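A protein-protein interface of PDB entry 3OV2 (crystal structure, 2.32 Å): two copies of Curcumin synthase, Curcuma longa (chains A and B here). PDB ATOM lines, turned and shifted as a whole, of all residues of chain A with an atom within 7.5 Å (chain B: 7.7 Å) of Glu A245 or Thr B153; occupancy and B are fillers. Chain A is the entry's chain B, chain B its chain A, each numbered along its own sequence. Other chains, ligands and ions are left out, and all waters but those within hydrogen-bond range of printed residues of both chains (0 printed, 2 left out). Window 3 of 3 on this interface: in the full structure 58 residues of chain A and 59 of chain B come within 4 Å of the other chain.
O of Leu B152 sits at hydrogen-bond distance from N of Thr A246, 3.0 Å away.
The side-chain amide oxygen of Gln A244 lies close to the backbone carbonyl oxygen of Val B154 (3.1 Å).
The side-chain amide oxygen (OD1) of Asn B155 is in hydrogen-bond range of the backbone NH (N) of Gln A244, at 3.4 Å.
N of Arg B156 is in hydrogen-bond range of OE1 of Gln A244 (2.6 Å).
The side-chain hydroxyl (OG1) of Thr A246 sits at hydrogen-bond distance from the guanidinium group (NH1) of Arg B156 (2.9 Å).
The guanidinium group (NH1) of Arg B156 is in hydrogen-bond range of the side-chain hydroxyl (OG) of Ser A378 (3.2 Å).
O of Thr B125 is in hydrogen-bond range of N of Asn B155 (2.9 Å).
A ring nitrogen (NE2) of His B126 lies within hydrogen-bond range of the side-chain amide nitrogen (ND2) of Asn B155 (3.2 Å).
The backbone carbonyl oxygen of Gln A244 is in hydrogen-bond range of the guanidinium group of Arg A285 (3.2 Å).
The side-chain carboxylate (OE2) of Glu A380 is in hydrogen-bond range of the side-chain amide nitrogen (NE2) of Gln A244 (2.9 Å).
OE1 of Glu A245 lies within salt-bridge range of NH2 of Arg A285 (3.5 Å).
The backbone NH (N) of Ile A379 lies within hydrogen-bond range of the backbone carbonyl oxygen (O) of Glu A245 (2.8 Å).
No position is printed for both chains.
Of the printed residues of chain B, Arg A172 touches Asn B155 and Arg B156.
Printed residues of chain B within 4 Å of Gln A244: Thr B153, Val B154, Asn B155 and Arg B156.
Of chain B, only Leu B152 (3.7 Å) and Thr B153 (3.4 Å) come within 4 Å of Glu A245.
Leu A279 touches none of the printed residues of chain B.
Gly A372 touches none of the printed residues of chain B.
Thr B153 touches just these residues of chain A: Gln A244, Glu A245 and Arg A285.
Of the printed residues of chain A, Arg B156 touches Arg A172, Gln A244, Thr A246 and Ser A378.
The nearest printed residue of chain B that does not touch Ser A378 is Leu B152 (7.9 Å).
Asn B155 touches Arg A172.
Arg A172 touches Arg B156 (NH2 to O, 3.6 Å).
Thr B153 touches Gln A244 (O to O, 3.6 Å).
O of Leu B152 touches CA of Glu A245 (3.7 Å).
Thr B153 touches Glu A245.
NH2 of Arg A285 touches CG2 of Thr B153, at 3.8 Å.
Printed residues of chain A that touch a printed residue of chain B: Arg A172, Gln A244, Glu A245, Thr A246, Arg A285 and Ser A378.
Of the 11 printed residues of chain B, 5 touch a printed residue of chain A.
Printed residues of chain B that touch a printed residue of chain A: Leu B152, Thr B153, Val B154, Asn B155 and Arg B156.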
ATOM      1  N   ARG A 172     -31.034  14.148   9.489  1.00  0.00           N
ATOM      2  CA  ARG A 172     -30.456  13.522  10.681  1.00  0.00           C
ATOM      3  C   ARG A 172     -31.527  12.835  11.511  1.00  0.00           C
ATOM      4  O   ARG A 172     -31.301  11.732  11.998  1.00  0.00           O
ATOM      5  CB  ARG A 172     -29.665  14.537  11.526  1.00  0.00           C
ATOM      6  CG  ARG A 172     -29.006  13.929  12.790  1.00  0.00           C
ATOM      7  CD  ARG A 172     -28.006  14.879  13.452  1.00  0.00           C
ATOM      8  NE  ARG A 172     -28.468  16.274  13.498  1.00  0.00           N
ATOM      9  CZ  ARG A 172     -29.140  16.840  14.504  1.00  0.00           C
ATOM     10  NH1 ARG A 172     -29.472  16.142  15.595  1.00  0.00           N
ATOM     11  NH2 ARG A 172     -29.493  18.118  14.409  1.00  0.00           N
ATOM     12  N   MET A 243     -24.454  14.308  11.449  1.00  0.00           N
ATOM     13  CA  MET A 243     -23.891  14.860  12.655  1.00  0.00           C
ATOM     14  C   MET A 243     -24.161  16.348  12.791  1.00  0.00           C
ATOM     15  O   MET A 243     -24.425  17.054  11.809  1.00  0.00           O
ATOM     16  CB  MET A 243     -22.382  14.595  12.691  1.00  0.00           C
ATOM     17  CG  MET A 243     -21.638  15.154  11.502  1.00  0.00           C
ATOM     18  SD  MET A 243     -20.075  14.302  11.186  1.00  0.00           S
ATOM     19  CE  MET A 243     -20.648  12.669  10.674  1.00  0.00           C
ATOM     20  N   GLN A 244     -24.077  16.817  14.026  1.00  0.00           N
ATOM     21  CA  GLN A 244     -24.208  18.237  14.322  1.00  0.00           C
ATOM     22  C   GLN A 244     -22.994  18.715  15.089  1.00  0.00           C
ATOM     23  O   GLN A 244     -22.443  17.983  15.908  1.00  0.00           O
ATOM     24  CB  GLN A 244     -25.460  18.491  15.146  1.00  0.00           C
ATOM     25  CG  GLN A 244     -25.730  19.955  15.391  1.00  0.00           C
ATOM     26  CD  GLN A 244     -26.854  20.185  16.372  1.00  0.00           C
ATOM     27  OE1 GLN A 244     -26.820  19.713  17.516  1.00  0.00           O
ATOM     28  NE2 GLN A 244     -27.853  20.937  15.939  1.00  0.00           N
ATOM     29  N   GLU A 245     -22.571  19.944  14.824  1.00  0.00           N
ATOM     30  CA  GLU A 245     -21.546  20.564  15.651  1.00  0.00           C
ATOM     31  C   GLU A 245     -21.935  22.003  15.901  1.00  0.00           C
ATOM     32  O   GLU A 245     -22.439  22.670  15.003  1.00  0.00           O
ATOM     33  CB  GLU A 245     -20.166  20.473  14.977  1.00  0.00           C
ATOM     34  CG  GLU A 245     -18.985  20.635  15.937  1.00  0.00           C
ATOM     35  CD  GLU A 245     -17.817  19.685  15.647  1.00  0.00           C
ATOM     36  OE1 GLU A 245     -18.056  18.492  15.311  1.00  0.00           O
ATOM     37  OE2 GLU A 245     -16.654  20.140  15.783  1.00  0.00           O
ATOM     38  N   THR A 246     -21.727  22.462  17.131  1.00  0.00           N
ATOM     39  CA  THR A 246     -21.888  23.873  17.480  1.00  0.00           C
ATOM     40  C   THR A 246     -20.511  24.527  17.637  1.00  0.00           C
ATOM     41  O   THR A 246     -19.618  23.990  18.295  1.00  0.00           O
ATOM     42  CB  THR A 246     -22.704  24.068  18.776  1.00  0.00           C
ATOM     43  OG1 THR A 246     -23.932  23.329  18.703  1.00  0.00           O
ATOM     44  CG2 THR A 246     -23.021  25.532  18.992  1.00  0.00           C
ATOM     45  N   VAL A 247     -20.354  25.698  17.040  1.00  0.00           N
ATOM     46  CA  VAL A 247     -19.089  26.428  17.094  1.00  0.00           C
ATOM     47  C   VAL A 247     -19.054  27.353  18.309  1.00  0.00           C
ATOM     48  O   VAL A 247     -19.860  28.280  18.412  1.00  0.00           O
ATOM     49  CB  VAL A 247     -18.864  27.222  15.780  1.00  0.00           C
ATOM     50  CG1 VAL A 247     -17.609  28.094  15.853  1.00  0.00           C
ATOM     51  CG2 VAL A 247     -18.801  26.260  14.598  1.00  0.00           C
ATOM     52  N   ALA A 248     -18.121  27.082  19.224  1.00  0.00           N
ATOM     53  CA  ALA A 248     -17.943  27.851  20.454  1.00  0.00           C
ATOM     54  C   ALA A 248     -18.033  29.355  20.233  1.00  0.00           C
ATOM     55  O   ALA A 248     -17.519  29.882  19.235  1.00  0.00           O
ATOM     56  CB  ALA A 248     -16.602  27.511  21.088  1.00  0.00           C
ATOM     57  N   ASN A 278     -14.794  27.250  10.093  1.00  0.00           N
ATOM     58  CA  ASN A 278     -15.194  26.301  11.128  1.00  0.00           C
ATOM     59  C   ASN A 278     -15.755  24.968  10.611  1.00  0.00           C
ATOM     60  O   ASN A 278     -16.339  24.188  11.370  1.00  0.00           O
ATOM     61  CB  ASN A 278     -16.137  26.981  12.118  1.00  0.00           C
ATOM     62  CG  ASN A 278     -15.397  27.902  13.079  1.00  0.00           C
ATOM     63  OD1 ASN A 278     -14.723  27.437  13.998  1.00  0.00           O
ATOM     64  ND2 ASN A 278     -15.525  29.212  12.874  1.00  0.00           N
ATOM     65  N   LEU A 279     -15.540  24.708   9.326  1.00  0.00           N
ATOM     66  CA  LEU A 279     -15.978  23.473   8.680  1.00  0.00           C
ATOM     67  C   LEU A 279     -15.016  22.298   8.871  1.00  0.00           C
ATOM     68  O   LEU A 279     -15.432  21.134   8.792  1.00  0.00           O
ATOM     69  CB  LEU A 279     -16.210  23.705   7.186  1.00  0.00           C
ATOM     70  CG  LEU A 279     -17.338  24.647   6.774  1.00  0.00           C
ATOM     71  CD1 LEU A 279     -17.292  24.854   5.274  1.00  0.00           C
ATOM     72  CD2 LEU A 279     -18.712  24.123   7.196  1.00  0.00           C
ATOM     73  N   GLY A 280     -13.743  22.608   9.120  1.00  0.00           N
ATOM     74  CA  GLY A 280     -12.690  21.598   9.251  1.00  0.00           C
ATOM     75  C   GLY A 280     -13.039  20.380  10.088  1.00  0.00           C
ATOM     76  O   GLY A 280     -12.938  19.250   9.607  1.00  0.00           O
ATOM     77  N   ARG A 281     -13.451  20.618  11.335  1.00  0.00           N
ATOM     78  CA  ARG A 281     -13.849  19.557  12.277  1.00  0.00           C
ATOM     79  C   ARG A 281     -14.962  18.662  11.749  1.00  0.00           C
ATOM     80  O   ARG A 281     -14.826  17.443  11.732  1.00  0.00           O
ATOM     81  CB  ARG A 281     -14.306  20.154  13.621  1.00  0.00           C
ATOM     82  CG  ARG A 281     -13.327  19.993  14.787  1.00  0.00           C
ATOM     83  CD  ARG A 281     -12.500  21.256  15.030  1.00  0.00           C
ATOM     84  NE  ARG A 281     -13.331  22.425  15.363  1.00  0.00           N
ATOM     85  CZ  ARG A 281     -13.516  23.480  14.562  1.00  0.00           C
ATOM     86  NH1 ARG A 281     -12.928  23.531  13.361  1.00  0.00           N
ATOM     87  NH2 ARG A 281     -14.290  24.486  14.960  1.00  0.00           N
ATOM     88  N   SER A 282     -16.067  19.280  11.343  1.00  0.00           N
ATOM     89  CA  SER A 282     -17.212  18.550  10.791  1.00  0.00           C
ATOM     90  C   SER A 282     -16.808  17.658   9.629  1.00  0.00           C
ATOM     91  O   SER A 282     -17.117  16.465   9.631  1.00  0.00           O
ATOM     92  CB  SER A 282     -18.318  19.508  10.348  1.00  0.00           C
ATOM     93  OG  SER A 282     -19.111  19.884  11.449  1.00  0.00           O
ATOM     94  N   LEU A 283     -16.097  18.227   8.659  1.00  0.00           N
ATOM     95  CA  LEU A 283     -15.691  17.477   7.466  1.00  0.00           C
ATOM     96  C   LEU A 283     -14.710  16.336   7.772  1.00  0.00           C
ATOM     97  O   LEU A 283     -14.755  15.286   7.137  1.00  0.00           O
ATOM     98  CB  LEU A 283     -15.135  18.421   6.402  1.00  0.00           C
ATOM     99  CG  LEU A 283     -16.128  19.482   5.916  1.00  0.00           C
ATOM    100  CD1 LEU A 283     -15.415  20.496   5.033  1.00  0.00           C
ATOM    101  CD2 LEU A 283     -17.323  18.850   5.194  1.00  0.00           C
ATOM    102  N   ARG A 285     -14.536  14.615  10.824  1.00  0.00           N
ATOM    103  CA  ARG A 285     -15.398  13.585  11.425  1.00  0.00           C
ATOM    104  C   ARG A 285     -16.145  12.805  10.340  1.00  0.00           C
ATOM    105  O   ARG A 285     -16.238  11.575  10.389  1.00  0.00           O
ATOM    106  CB  ARG A 285     -16.417  14.205  12.399  1.00  0.00           C
ATOM    107  CG  ARG A 285     -15.998  14.230  13.874  1.00  0.00           C
ATOM    108  CD  ARG A 285     -17.160  13.820  14.825  1.00  0.00           C
ATOM    109  NE  ARG A 285     -18.158  14.883  15.009  1.00  0.00           N
ATOM    110  CZ  ARG A 285     -19.405  14.704  15.459  1.00  0.00           C
ATOM    111  NH1 ARG A 285     -19.850  13.494  15.776  1.00  0.00           N
ATOM    112  NH2 ARG A 285     -20.218  15.744  15.587  1.00  0.00           N
ATOM    113  N   GLY A 372     -25.759  22.021   6.067  1.00  0.00           N
ATOM    114  CA  GLY A 372     -26.527  23.148   6.538  1.00  0.00           C
ATOM    115  C   GLY A 372     -25.814  23.855   7.677  1.00  0.00           C
ATOM    116  O   GLY A 372     -25.065  23.244   8.442  1.00  0.00           O
ATOM    117  N   GLY A 374     -26.565  27.414  10.435  1.00  0.00           N
ATOM    118  CA  GLY A 374     -27.420  28.488  10.918  1.00  0.00           C
ATOM    119  C   GLY A 374     -27.035  28.932  12.321  1.00  0.00           C
ATOM    120  O   GLY A 374     -25.969  28.568  12.808  1.00  0.00           O
ATOM    121  N   PRO A 375     -27.895  29.749  12.957  1.00  0.00           N
ATOM    122  CA  PRO A 375     -27.780  30.178  14.342  1.00  0.00           C
ATOM    123  C   PRO A 375     -27.230  29.107  15.272  1.00  0.00           C
ATOM    124  O   PRO A 375     -27.695  27.963  15.289  1.00  0.00           O
ATOM    125  CB  PRO A 375     -29.227  30.535  14.701  1.00  0.00           C
ATOM    126  CG  PRO A 375     -29.756  31.147  13.435  1.00  0.00           C
ATOM    127  CD  PRO A 375     -28.955  30.519  12.267  1.00  0.00           C
ATOM    128  N   GLY A 376     -26.231  29.512  16.035  1.00  0.00           N
ATOM    129  CA  GLY A 376     -25.510  28.639  16.937  1.00  0.00           C
ATOM    130  C   GLY A 376     -24.165  29.301  17.219  1.00  0.00           C
ATOM    131  O   GLY A 376     -23.974  29.861  18.299  1.00  0.00           O
ATOM    132  N   LEU A 377     -23.234  29.279  16.259  1.00  0.00           N
ATOM    133  CA  LEU A 377     -23.423  28.716  14.917  1.00  0.00           C
ATOM    134  C   LEU A 377     -23.599  27.204  14.916  1.00  0.00           C
ATOM    135  O   LEU A 377     -22.859  26.491  15.597  1.00  0.00           O
ATOM    136  CB  LEU A 377     -22.239  29.102  14.021  1.00  0.00           C
ATOM    137  CG  LEU A 377     -22.453  28.988  12.508  1.00  0.00           C
ATOM    138  CD1 LEU A 377     -23.343  30.107  11.982  1.00  0.00           C
ATOM    139  CD2 LEU A 377     -21.084  29.011  11.813  1.00  0.00           C
ATOM    140  N   SER A 378     -24.595  26.728  14.163  1.00  0.00           N
ATOM    141  CA  SER A 378     -24.884  25.297  14.054  1.00  0.00           C
ATOM    142  C   SER A 378     -24.454  24.779  12.691  1.00  0.00           C
ATOM    143  O   SER A 378     -24.773  25.395  11.670  1.00  0.00           O
ATOM    144  CB  SER A 378     -26.382  25.022  14.232  1.00  0.00           C
ATOM    145  OG  SER A 378     -26.858  25.562  15.448  1.00  0.00           O
ATOM    146  N   ILE A 379     -23.725  23.664  12.681  1.00  0.00           N
ATOM    147  CA  ILE A 379     -23.287  23.029  11.424  1.00  0.00           C
ATOM    148  C   ILE A 379     -23.852  21.639  11.288  1.00  0.00           C
ATOM    149  O   ILE A 379     -23.545  20.770  12.094  1.00  0.00           O
ATOM    150  CB  ILE A 379     -21.733  22.878  11.308  1.00  0.00           C
ATOM    151  CG1 ILE A 379     -20.993  24.169  11.706  1.00  0.00           C
ATOM    152  CG2 ILE A 379     -21.360  22.375   9.914  1.00  0.00           C
ATOM    153  CD1 ILE A 379     -21.318  25.372  10.854  1.00  0.00           C
ATOM    154  N   GLU A 380     -24.642  21.427  10.245  1.00  0.00           N
ATOM    155  CA  GLU A 380     -25.225  20.118   9.974  1.00  0.00           C
ATOM    156  C   GLU A 380     -24.513  19.484   8.780  1.00  0.00           C
ATOM    157  O   GLU A 380     -24.492  20.048   7.687  1.00  0.00           O
ATOM    158  CB  GLU A 380     -26.735  20.239   9.734  1.00  0.00           C
ATOM    159  CG  GLU A 380     -27.523  20.861  10.909  1.00  0.00           C
ATOM    160  CD  GLU A 380     -27.849  19.876  12.038  1.00  0.00           C
ATOM    161  OE1 GLU A 380     -27.718  18.651  11.846  1.00  0.00           O
ATOM    162  OE2 GLU A 380     -28.255  20.336  13.135  1.00  0.00           O
ATOM    163  N   THR A 381     -23.906  18.322   9.017  1.00  0.00           N
ATOM    164  CA  THR A 381     -23.204  17.567   7.986  1.00  0.00           C
ATOM    165  C   THR A 381     -23.879  16.210   7.800  1.00  0.00           C
ATOM    166  O   THR A 381     -24.071  15.448   8.755  1.00  0.00           O
ATOM    167  CB  THR A 381     -21.718  17.363   8.351  1.00  0.00           C
ATOM    168  OG1 THR A 381     -21.140  18.626   8.696  1.00  0.00           O
ATOM    169  CG2 THR A 381     -20.911  16.739   7.164  1.00  0.00           C
ATOM    170  N   SER B 122     -19.987  14.261  29.513  1.00  0.00           N
ATOM    171  CA  SER B 122     -19.325  14.100  28.214  1.00  0.00           C
ATOM    172  C   SER B 122     -19.816  12.864  27.452  1.00  0.00           C
ATOM    173  O   SER B 122     -19.630  12.749  26.247  1.00  0.00           O
ATOM    174  CB  SER B 122     -17.802  14.049  28.392  1.00  0.00           C
ATOM    175  OG  SER B 122     -17.415  12.954  29.217  1.00  0.00           O
ATOM    176  N   ILE B 124     -23.028  12.174  27.242  1.00  0.00           N
ATOM    177  CA  ILE B 124     -24.317  12.549  26.621  1.00  0.00           C
ATOM    178  C   ILE B 124     -24.102  12.814  25.139  1.00  0.00           C
ATOM    179  O   ILE B 124     -23.246  13.616  24.784  1.00  0.00           O
ATOM    180  CB  ILE B 124     -24.924  13.800  27.310  1.00  0.00           C
ATOM    181  CG1 ILE B 124     -25.357  13.443  28.737  1.00  0.00           C
ATOM    182  CG2 ILE B 124     -26.089  14.402  26.507  1.00  0.00           C
ATOM    183  CD1 ILE B 124     -25.902  14.611  29.520  1.00  0.00           C
ATOM    184  N   THR B 125     -24.855  12.140  24.268  1.00  0.00           N
ATOM    185  CA  THR B 125     -24.646  12.287  22.816  1.00  0.00           C
ATOM    186  C   THR B 125     -25.715  13.141  22.148  1.00  0.00           C
ATOM    187  O   THR B 125     -25.455  13.784  21.119  1.00  0.00           O
ATOM    188  CB  THR B 125     -24.587  10.920  22.075  1.00  0.00           C
ATOM    189  OG1 THR B 125     -25.788  10.170  22.331  1.00  0.00           O
ATOM    190  CG2 THR B 125     -23.347  10.118  22.486  1.00  0.00           C
ATOM    191  N   HIS B 126     -26.914  13.126  22.737  1.00  0.00           N
ATOM    192  CA  HIS B 126     -28.087  13.830  22.208  1.00  0.00           C
ATOM    193  C   HIS B 126     -28.808  14.638  23.303  1.00  0.00           C
ATOM    194  O   HIS B 126     -28.873  14.224  24.473  1.00  0.00           O
ATOM    195  CB  HIS B 126     -29.103  12.858  21.592  1.00  0.00           C
ATOM    196  CG  HIS B 126     -28.584  12.033  20.451  1.00  0.00           C
ATOM    197  ND1 HIS B 126     -27.673  11.008  20.620  1.00  0.00           N
ATOM    198  CD2 HIS B 126     -28.902  12.039  19.133  1.00  0.00           C
ATOM    199  CE1 HIS B 126     -27.422  10.450  19.450  1.00  0.00           C
ATOM    200  NE2 HIS B 126     -28.155  11.058  18.530  1.00  0.00           N
ATOM    201  N   LEU B 150     -22.635  21.201  28.123  1.00  0.00           N
ATOM    202  CA  LEU B 150     -22.587  20.019  27.275  1.00  0.00           C
ATOM    203  C   LEU B 150     -21.504  20.165  26.199  1.00  0.00           C
ATOM    204  O   LEU B 150     -21.249  21.276  25.738  1.00  0.00           O
ATOM    205  CB  LEU B 150     -23.964  19.737  26.651  1.00  0.00           C
ATOM    206  CG  LEU B 150     -25.113  19.336  27.607  1.00  0.00           C
ATOM    207  CD1 LEU B 150     -26.346  18.871  26.840  1.00  0.00           C
ATOM    208  CD2 LEU B 150     -24.702  18.286  28.646  1.00  0.00           C
ATOM    209  N   PRO B 151     -20.847  19.051  25.807  1.00  0.00           N
ATOM    210  CA  PRO B 151     -19.892  19.157  24.700  1.00  0.00           C
ATOM    211  C   PRO B 151     -20.550  19.677  23.416  1.00  0.00           C
ATOM    212  O   PRO B 151     -21.750  19.455  23.187  1.00  0.00           O
ATOM    213  CB  PRO B 151     -19.369  17.725  24.518  1.00  0.00           C
ATOM    214  CG  PRO B 151     -20.241  16.851  25.361  1.00  0.00           C
ATOM    215  CD  PRO B 151     -20.834  17.714  26.425  1.00  0.00           C
ATOM    216  N   LEU B 152     -19.753  20.367  22.601  1.00  0.00           N
ATOM    217  CA  LEU B 152     -20.251  21.087  21.428  1.00  0.00           C
ATOM    218  C   LEU B 152     -20.738  20.151  20.327  1.00  0.00           C
ATOM    219  O   LEU B 152     -21.402  20.589  19.392  1.00  0.00           O
ATOM    220  CB  LEU B 152     -19.172  22.039  20.882  1.00  0.00           C
ATOM    221  CG  LEU B 152     -18.490  22.953  21.912  1.00  0.00           C
ATOM    222  CD1 LEU B 152     -17.128  23.436  21.397  1.00  0.00           C
ATOM    223  CD2 LEU B 152     -19.392  24.125  22.337  1.00  0.00           C
ATOM    224  N   THR B 153     -20.399  18.873  20.447  1.00  0.00           N
ATOM    225  CA  THR B 153     -20.773  17.874  19.463  1.00  0.00           C
ATOM    226  C   THR B 153     -22.101  17.183  19.812  1.00  0.00           C
ATOM    227  O   THR B 153     -22.558  16.331  19.050  1.00  0.00           O
ATOM    228  CB  THR B 153     -19.664  16.795  19.286  1.00  0.00           C
ATOM    229  OG1 THR B 153     -19.226  16.350  20.578  1.00  0.00           O
ATOM    230  CG2 THR B 153     -18.455  17.344  18.520  1.00  0.00           C
ATOM    231  N   VAL B 154     -22.715  17.527  20.948  1.00  0.00           N
ATOM    232  CA  VAL B 154     -24.034  16.949  21.294  1.00  0.00           C
ATOM    233  C   VAL B 154     -25.072  17.308  20.228  1.00  0.00           C
ATOM    234  O   VAL B 154     -25.222  18.477  19.859  1.00  0.00           O
ATOM    235  CB  VAL B 154     -24.543  17.373  22.698  1.00  0.00           C
ATOM    236  CG1 VAL B 154     -26.036  17.040  22.866  1.00  0.00           C
ATOM    237  CG2 VAL B 154     -23.750  16.667  23.797  1.00  0.00           C
ATOM    238  N   ASN B 155     -25.755  16.290  19.713  1.00  0.00           N
ATOM    239  CA  ASN B 155     -26.821  16.485  18.733  1.00  0.00           C
ATOM    240  C   ASN B 155     -28.033  17.113  19.418  1.00  0.00           C
ATOM    241  O   ASN B 155     -28.720  16.452  20.185  1.00  0.00           O
ATOM    242  CB  ASN B 155     -27.219  15.151  18.069  1.00  0.00           C
ATOM    243  CG  ASN B 155     -26.030  14.415  17.426  1.00  0.00           C
ATOM    244  OD1 ASN B 155     -25.243  15.001  16.674  1.00  0.00           O
ATOM    245  ND2 ASN B 155     -25.913  13.120  17.714  1.00  0.00           N
ATOM    246  N   ARG B 156     -28.282  18.386  19.133  1.00  0.00           N
ATOM    247  CA  ARG B 156     -29.370  19.129  19.742  1.00  0.00           C
ATOM    248  C   ARG B 156     -30.618  19.111  18.859  1.00  0.00           C
ATOM    249  O   ARG B 156     -30.525  19.195  17.631  1.00  0.00           O
ATOM    250  CB  ARG B 156     -28.974  20.595  19.936  1.00  0.00           C
ATOM    251  CG  ARG B 156     -27.848  20.930  20.915  1.00  0.00           C
ATOM    252  CD  ARG B 156     -27.244  22.325  20.530  1.00  0.00           C
ATOM    253  NE  ARG B 156     -28.230  23.152  19.817  1.00  0.00           N
ATOM    254  CZ  ARG B 156     -27.974  23.946  18.781  1.00  0.00           C
ATOM    255  NH1 ARG B 156     -26.731  24.092  18.307  1.00  0.00           N
ATOM    256  NH2 ARG B 156     -28.979  24.608  18.212  1.00  0.00           N
